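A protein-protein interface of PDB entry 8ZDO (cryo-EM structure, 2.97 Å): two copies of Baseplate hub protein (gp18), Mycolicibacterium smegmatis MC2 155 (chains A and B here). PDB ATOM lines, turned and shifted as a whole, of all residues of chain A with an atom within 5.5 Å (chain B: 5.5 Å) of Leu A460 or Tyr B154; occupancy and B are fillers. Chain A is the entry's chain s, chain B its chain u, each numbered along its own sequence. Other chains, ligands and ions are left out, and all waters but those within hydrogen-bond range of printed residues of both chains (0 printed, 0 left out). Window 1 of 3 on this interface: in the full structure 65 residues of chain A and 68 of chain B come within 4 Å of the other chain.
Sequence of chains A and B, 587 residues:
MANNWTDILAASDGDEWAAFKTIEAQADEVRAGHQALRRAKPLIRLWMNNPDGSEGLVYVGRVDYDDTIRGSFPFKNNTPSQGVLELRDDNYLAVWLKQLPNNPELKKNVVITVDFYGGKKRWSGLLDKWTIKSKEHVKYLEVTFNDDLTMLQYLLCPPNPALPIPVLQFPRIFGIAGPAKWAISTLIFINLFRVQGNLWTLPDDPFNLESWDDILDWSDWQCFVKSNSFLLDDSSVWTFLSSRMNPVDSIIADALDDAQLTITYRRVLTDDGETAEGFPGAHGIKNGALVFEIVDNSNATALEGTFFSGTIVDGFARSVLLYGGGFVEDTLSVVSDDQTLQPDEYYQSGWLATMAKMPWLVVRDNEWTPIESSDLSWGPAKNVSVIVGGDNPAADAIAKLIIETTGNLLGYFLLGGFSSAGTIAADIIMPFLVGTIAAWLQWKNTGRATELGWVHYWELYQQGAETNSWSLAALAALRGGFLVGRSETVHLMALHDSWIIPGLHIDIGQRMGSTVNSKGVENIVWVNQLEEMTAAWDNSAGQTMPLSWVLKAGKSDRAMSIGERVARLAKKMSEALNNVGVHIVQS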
ATOM      1  N   LYS A 382      -8.200  -4.017  24.434  1.00  0.00           N
ATOM      2  CA  LYS A 382      -9.454  -3.537  23.872  1.00  0.00           C
ATOM      3  C   LYS A 382     -10.658  -3.836  24.755  1.00  0.00           C
ATOM      4  O   LYS A 382     -11.312  -2.908  25.234  1.00  0.00           O
ATOM      5  CB  LYS A 382      -9.663  -4.143  22.479  1.00  0.00           C
ATOM      6  CG  LYS A 382      -8.416  -4.182  21.621  1.00  0.00           C
ATOM      7  CD  LYS A 382      -8.137  -2.830  21.003  1.00  0.00           C
ATOM      8  CE  LYS A 382      -8.973  -2.610  19.760  1.00  0.00           C
ATOM      9  NZ  LYS A 382      -8.295  -1.708  18.791  1.00  0.00           N
ATOM     10  N   ASN A 383     -10.947  -5.103  25.025  1.00  0.00           N
ATOM     11  CA  ASN A 383     -12.202  -5.494  25.650  1.00  0.00           C
ATOM     12  C   ASN A 383     -11.963  -5.879  27.101  1.00  0.00           C
ATOM     13  O   ASN A 383     -11.096  -6.706  27.396  1.00  0.00           O
ATOM     14  CB  ASN A 383     -12.861  -6.649  24.890  1.00  0.00           C
ATOM     15  CG  ASN A 383     -11.999  -7.888  24.851  1.00  0.00           C
ATOM     16  OD1 ASN A 383     -10.849  -7.842  24.424  1.00  0.00           O
ATOM     17  ND2 ASN A 383     -12.551  -9.006  25.303  1.00  0.00           N
ATOM     18  N   SER A 385     -14.208  -7.348  29.123  1.00  0.00           N
ATOM     19  CA  SER A 385     -14.864  -8.592  29.492  1.00  0.00           C
ATOM     20  C   SER A 385     -15.026  -9.508  28.288  1.00  0.00           C
ATOM     21  O   SER A 385     -15.107  -9.063  27.139  1.00  0.00           O
ATOM     22  CB  SER A 385     -16.231  -8.330  30.135  1.00  0.00           C
ATOM     23  OG  SER A 385     -16.964  -7.372  29.400  1.00  0.00           O
ATOM     24  N   VAL A 386     -15.072 -10.804  28.576  1.00  0.00           N
ATOM     25  CA  VAL A 386     -15.244 -11.829  27.559  1.00  0.00           C
ATOM     26  C   VAL A 386     -16.408 -12.723  27.959  1.00  0.00           C
ATOM     27  O   VAL A 386     -16.611 -13.017  29.144  1.00  0.00           O
ATOM     28  CB  VAL A 386     -13.956 -12.659  27.348  1.00  0.00           C
ATOM     29  CG1 VAL A 386     -13.610 -13.456  28.589  1.00  0.00           C
ATOM     30  CG2 VAL A 386     -14.094 -13.568  26.144  1.00  0.00           C
ATOM     31  N   ILE A 387     -17.185 -13.135  26.962  1.00  0.00           N
ATOM     32  CA  ILE A 387     -18.274 -14.088  27.127  1.00  0.00           C
ATOM     33  C   ILE A 387     -17.973 -15.294  26.253  1.00  0.00           C
ATOM     34  O   ILE A 387     -17.708 -15.150  25.054  1.00  0.00           O
ATOM     35  CB  ILE A 387     -19.635 -13.471  26.760  1.00  0.00           C
ATOM     36  CG1 ILE A 387     -19.969 -12.318  27.704  1.00  0.00           C
ATOM     37  CG2 ILE A 387     -20.724 -14.523  26.807  1.00  0.00           C
ATOM     38  CD1 ILE A 387     -21.254 -11.609  27.371  1.00  0.00           C
ATOM     39  N   TYR A 457     -13.633  -0.281  25.564  1.00  0.00           N
ATOM     40  CA  TYR A 457     -14.528  -1.226  24.915  1.00  0.00           C
ATOM     41  C   TYR A 457     -14.998  -2.253  25.935  1.00  0.00           C
ATOM     42  O   TYR A 457     -14.237  -2.674  26.809  1.00  0.00           O
ATOM     43  CB  TYR A 457     -13.830  -1.919  23.750  1.00  0.00           C
ATOM     44  CG  TYR A 457     -13.410  -0.988  22.639  1.00  0.00           C
ATOM     45  CD1 TYR A 457     -14.271  -0.011  22.161  1.00  0.00           C
ATOM     46  CD2 TYR A 457     -12.154  -1.091  22.064  1.00  0.00           C
ATOM     47  CE1 TYR A 457     -13.888   0.837  21.148  1.00  0.00           C
ATOM     48  CE2 TYR A 457     -11.765  -0.249  21.050  1.00  0.00           C
ATOM     49  CZ  TYR A 457     -12.635   0.712  20.594  1.00  0.00           C
ATOM     50  OH  TYR A 457     -12.247   1.556  19.582  1.00  0.00           O
ATOM     51  N   TRP A 458     -16.262  -2.654  25.825  1.00  0.00           N
ATOM     52  CA  TRP A 458     -16.896  -3.370  26.925  1.00  0.00           C
ATOM     53  C   TRP A 458     -16.560  -4.854  26.920  1.00  0.00           C
ATOM     54  O   TRP A 458     -15.904  -5.355  27.840  1.00  0.00           O
ATOM     55  CB  TRP A 458     -18.411  -3.180  26.862  1.00  0.00           C
ATOM     56  CG  TRP A 458     -18.853  -1.790  27.131  1.00  0.00           C
ATOM     57  CD1 TRP A 458     -18.867  -1.154  28.331  1.00  0.00           C
ATOM     58  CD2 TRP A 458     -19.352  -0.855  26.174  1.00  0.00           C
ATOM     59  NE1 TRP A 458     -19.353   0.117  28.186  1.00  0.00           N
ATOM     60  CE2 TRP A 458     -19.656   0.327  26.867  1.00  0.00           C
ATOM     61  CE3 TRP A 458     -19.573  -0.904  24.796  1.00  0.00           C
ATOM     62  CZ2 TRP A 458     -20.166   1.451  26.233  1.00  0.00           C
ATOM     63  CZ3 TRP A 458     -20.080   0.208  24.169  1.00  0.00           C
ATOM     64  CH2 TRP A 458     -20.370   1.372  24.885  1.00  0.00           C
ATOM     65  N   GLU A 459     -16.989  -5.570  25.887  1.00  0.00           N
ATOM     66  CA  GLU A 459     -17.033  -7.019  25.960  1.00  0.00           C
ATOM     67  C   GLU A 459     -16.872  -7.618  24.575  1.00  0.00           C
ATOM     68  O   GLU A 459     -17.023  -6.944  23.556  1.00  0.00           O
ATOM     69  CB  GLU A 459     -18.340  -7.498  26.600  1.00  0.00           C
ATOM     70  CG  GLU A 459     -19.584  -7.021  25.880  1.00  0.00           C
ATOM     71  CD  GLU A 459     -20.851  -7.298  26.657  1.00  0.00           C
ATOM     72  OE1 GLU A 459     -20.760  -7.872  27.762  1.00  0.00           O
ATOM     73  OE2 GLU A 459     -21.939  -6.930  26.169  1.00  0.00           O
ATOM     74  N   LEU A 460     -16.543  -8.903  24.563  1.00  0.00           N
ATOM     75  CA  LEU A 460     -16.346  -9.630  23.321  1.00  0.00           C
ATOM     76  C   LEU A 460     -16.784 -11.070  23.526  1.00  0.00           C
ATOM     77  O   LEU A 460     -16.506 -11.660  24.570  1.00  0.00           O
ATOM     78  CB  LEU A 460     -14.881  -9.569  22.891  1.00  0.00           C
ATOM     79  CG  LEU A 460     -14.513  -9.542  21.414  1.00  0.00           C
ATOM     80  CD1 LEU A 460     -15.134  -8.347  20.728  1.00  0.00           C
ATOM     81  CD2 LEU A 460     -13.005  -9.480  21.317  1.00  0.00           C
ATOM     82  N   TYR A 461     -17.474 -11.629  22.538  1.00  0.00           N
ATOM     83  CA  TYR A 461     -17.817 -13.042  22.565  1.00  0.00           C
ATOM     84  C   TYR A 461     -16.718 -13.832  21.873  1.00  0.00           C
ATOM     85  O   TYR A 461     -16.318 -13.500  20.754  1.00  0.00           O
ATOM     86  CB  TYR A 461     -19.159 -13.315  21.890  1.00  0.00           C
ATOM     87  CG  TYR A 461     -19.434 -14.793  21.738  1.00  0.00           C
ATOM     88  CD1 TYR A 461     -19.862 -15.550  22.815  1.00  0.00           C
ATOM     89  CD2 TYR A 461     -19.250 -15.433  20.522  1.00  0.00           C
ATOM     90  CE1 TYR A 461     -20.104 -16.897  22.686  1.00  0.00           C
ATOM     91  CE2 TYR A 461     -19.489 -16.782  20.386  1.00  0.00           C
ATOM     92  CZ  TYR A 461     -19.916 -17.508  21.471  1.00  0.00           C
ATOM     93  OH  TYR A 461     -20.160 -18.853  21.340  1.00  0.00           O
ATOM     94  N   GLN A 462     -16.236 -14.876  22.537  1.00  0.00           N
ATOM     95  CA  GLN A 462     -15.142 -15.685  22.021  1.00  0.00           C
ATOM     96  C   GLN A 462     -15.602 -17.121  21.834  1.00  0.00           C
ATOM     97  O   GLN A 462     -16.198 -17.713  22.739  1.00  0.00           O
ATOM     98  CB  GLN A 462     -13.932 -15.630  22.951  1.00  0.00           C
ATOM     99  CG  GLN A 462     -13.078 -14.395  22.752  1.00  0.00           C
ATOM    100  CD  GLN A 462     -12.733 -14.162  21.298  1.00  0.00           C
ATOM    101  OE1 GLN A 462     -12.089 -14.994  20.662  1.00  0.00           O
ATOM    102  NE2 GLN A 462     -13.164 -13.028  20.762  1.00  0.00           N
ATOM    103  N   VAL A 484      -7.201 -12.689  23.345  1.00  0.00           N
ATOM    104  CA  VAL A 484      -7.458 -12.020  22.072  1.00  0.00           C
ATOM    105  C   VAL A 484      -7.152 -10.529  22.140  1.00  0.00           C
ATOM    106  O   VAL A 484      -6.216 -10.048  21.493  1.00  0.00           O
ATOM    107  CB  VAL A 484      -8.911 -12.250  21.620  1.00  0.00           C
ATOM    108  CG1 VAL A 484      -9.240 -11.379  20.422  1.00  0.00           C
ATOM    109  CG2 VAL A 484      -9.135 -13.713  21.289  1.00  0.00           C
ATOM    110  N   GLY A 485      -7.931  -9.785  22.921  1.00  0.00           N
ATOM    111  CA  GLY A 485      -7.817  -8.340  22.913  1.00  0.00           C
ATOM    112  C   GLY A 485      -6.900  -7.772  23.974  1.00  0.00           C
ATOM    113  O   GLY A 485      -7.348  -7.018  24.842  1.00  0.00           O
ATOM    114  N   THR B 150     -17.036   2.108  16.784  1.00  0.00           N
ATOM    115  CA  THR B 150     -16.504   0.789  17.100  1.00  0.00           C
ATOM    116  C   THR B 150     -17.017   0.260  18.431  1.00  0.00           C
ATOM    117  O   THR B 150     -16.877  -0.935  18.699  1.00  0.00           O
ATOM    118  CB  THR B 150     -14.979   0.832  17.118  1.00  0.00           C
ATOM    119  OG1 THR B 150     -14.546   1.868  18.007  1.00  0.00           O
ATOM    120  CG2 THR B 150     -14.444   1.122  15.734  1.00  0.00           C
ATOM    121  N   MET B 151     -17.600   1.120  19.267  1.00  0.00           N
ATOM    122  CA  MET B 151     -18.170   0.660  20.528  1.00  0.00           C
ATOM    123  C   MET B 151     -19.317  -0.313  20.300  1.00  0.00           C
ATOM    124  O   MET B 151     -19.567  -1.192  21.133  1.00  0.00           O
ATOM    125  CB  MET B 151     -18.647   1.857  21.348  1.00  0.00           C
ATOM    126  CG  MET B 151     -17.538   2.785  21.811  1.00  0.00           C
ATOM    127  SD  MET B 151     -16.872   2.336  23.421  1.00  0.00           S
ATOM    128  CE  MET B 151     -15.617   3.591  23.621  1.00  0.00           C
ATOM    129  N   LEU B 152     -20.029  -0.174  19.184  1.00  0.00           N
ATOM    130  CA  LEU B 152     -21.146  -1.064  18.906  1.00  0.00           C
ATOM    131  C   LEU B 152     -20.687  -2.465  18.532  1.00  0.00           C
ATOM    132  O   LEU B 152     -21.453  -3.418  18.697  1.00  0.00           O
ATOM    133  CB  LEU B 152     -22.017  -0.475  17.800  1.00  0.00           C
ATOM    134  CG  LEU B 152     -22.599   0.898  18.135  1.00  0.00           C
ATOM    135  CD1 LEU B 152     -23.367   1.458  16.955  1.00  0.00           C
ATOM    136  CD2 LEU B 152     -23.487   0.817  19.361  1.00  0.00           C
ATOM    137  N   GLN B 153     -19.458  -2.612  18.032  1.00  0.00           N
ATOM    138  CA  GLN B 153     -18.918  -3.947  17.797  1.00  0.00           C
ATOM    139  C   GLN B 153     -18.641  -4.671  19.105  1.00  0.00           C
ATOM    140  O   GLN B 153     -18.772  -5.897  19.173  1.00  0.00           O
ATOM    141  CB  GLN B 153     -17.643  -3.864  16.962  1.00  0.00           C
ATOM    142  CG  GLN B 153     -17.809  -3.165  15.634  1.00  0.00           C
ATOM    143  CD  GLN B 153     -16.514  -3.093  14.858  1.00  0.00           C
ATOM    144  OE1 GLN B 153     -15.434  -3.012  15.441  1.00  0.00           O
ATOM    145  NE2 GLN B 153     -16.613  -3.129  13.536  1.00  0.00           N
ATOM    146  N   TYR B 154     -18.252  -3.936  20.142  1.00  0.00           N
ATOM    147  CA  TYR B 154     -17.956  -4.515  21.442  1.00  0.00           C
ATOM    148  C   TYR B 154     -19.156  -4.527  22.374  1.00  0.00           C
ATOM    149  O   TYR B 154     -19.063  -5.082  23.471  1.00  0.00           O
ATOM    150  CB  TYR B 154     -16.799  -3.761  22.093  1.00  0.00           C
ATOM    151  CG  TYR B 154     -15.509  -3.910  21.326  1.00  0.00           C
ATOM    152  CD1 TYR B 154     -15.226  -3.087  20.249  1.00  0.00           C
ATOM    153  CD2 TYR B 154     -14.584  -4.883  21.668  1.00  0.00           C
ATOM    154  CE1 TYR B 154     -14.057  -3.222  19.540  1.00  0.00           C
ATOM    155  CE2 TYR B 154     -13.410  -5.024  20.963  1.00  0.00           C
ATOM    156  CZ  TYR B 154     -13.152  -4.190  19.901  1.00  0.00           C
ATOM    157  OH  TYR B 154     -11.983  -4.323  19.191  1.00  0.00           O
ATOM    158  N   LEU B 155     -20.262  -3.913  21.979  1.00  0.00           N
ATOM    159  CA  LEU B 155     -21.520  -4.064  22.696  1.00  0.00           C
ATOM    160  C   LEU B 155     -22.231  -5.318  22.201  1.00  0.00           C
ATOM    161  O   LEU B 155     -22.499  -5.451  21.003  1.00  0.00           O
ATOM    162  CB  LEU B 155     -22.400  -2.831  22.504  1.00  0.00           C
ATOM    163  CG  LEU B 155     -23.479  -2.597  23.558  1.00  0.00           C
ATOM    164  CD1 LEU B 155     -22.855  -2.352  24.917  1.00  0.00           C
ATOM    165  CD2 LEU B 155     -24.351  -1.431  23.151  1.00  0.00           C
ATOM    166  N   LEU B 156     -22.538  -6.230  23.118  1.00  0.00           N
ATOM    167  CA  LEU B 156     -23.230  -7.472  22.811  1.00  0.00           C
ATOM    168  C   LEU B 156     -24.663  -7.415  23.323  1.00  0.00           C
ATOM    169  O   LEU B 156     -24.983  -6.675  24.256  1.00  0.00           O
ATOM    170  CB  LEU B 156     -22.522  -8.677  23.439  1.00  0.00           C
ATOM    171  CG  LEU B 156     -21.185  -9.137  22.867  1.00  0.00           C
ATOM    172  CD1 LEU B 156     -20.663 -10.309  23.668  1.00  0.00           C
ATOM    173  CD2 LEU B 156     -21.328  -9.510  21.405  1.00  0.00           C
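OH of Tyr A457 sits at hydrogen-bond distance from OG1 of Thr B150 (2.8 Å).
The backbone carbonyl oxygen (O) of Tyr B154 sits close to the backbone NH (N) of Glu A459, at 3.2 Å.
The side-chain carboxylate (OE2) of Glu A459 is in hydrogen-bond range of the backbone NH (N) of Leu B156 (3.2 Å).
No position is printed for both chains.
The backbone NH (N) of Lys A382 sits at hydrogen-bond distance from the backbone carbonyl oxygen (O) of Gly A485, 3.1 Å away.
The backbone carbonyl oxygen (O) of Trp A458 lies within hydrogen-bond range of the side-chain hydroxyl (OG) of Ser A385 (2.8 Å).
The backbone carbonyl oxygen of Ser A385 is in hydrogen-bond range of the backbone NH of Leu A460 (3.0 Å).
N of Ile A387 is in hydrogen-bond range of O of Leu A460.
N of Gln A462 is in hydrogen-bond range of O of Ile A387 (2.9 Å).
Hydrophobic or aromatic side chains of chain B within 4 Å of the printed part of chain A: Met B151, Tyr B154, Leu B155 and Leu B156.
Printed residues of chain A that touch a printed residue of chain B: Lys A382, Ile A387, Tyr A457, Trp A458, Glu A459, Leu A460 and Tyr A461.
OH of Tyr B154 touches CE of Lys A382, 3.5 Å away.
Leu B156 touches Ile A387 (CD1 to CD1, 3.97 Å).
Tyr A457 touches Met B151 (CD1 to SD, 3.7 Å).
CB of Tyr A457 touches CG of Tyr B154, at 3.6 Å.
CZ3 of Trp A458 touches O of Met B151, 3.4 Å away.
N of Trp A458 touches CB of Tyr B154, 3.9 Å away.
Leu B155 touches Trp A458.
CD1 of Leu A460 touches CD2 of Tyr B154, at 3.6 Å.
Leu B156 touches Leu A460 (CD1 to C, 3.96 Å).
Tyr A461 touches Leu B156 (N to CD1, 3.6 Å).
Val A386 touches none of the printed residues of chain B.
Printed residues of chain B within 4 Å of Tyr A457: Thr B150, Met B151 and Tyr B154.
Of the printed residues of chain B, Glu A459 touches Tyr B154 and Leu B156.
Leu A460 touches two residues of chain B.
Gln B153 touches none of the printed residues of chain A.
Tyr B154 touches five residues of chain A.
The nearest residue of chain B that does not touch Leu A460 is Gln B153 (4.7 Å).
The nearest residue of chain A that does not touch Tyr B154 is Asn A383 (4.1 Å).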
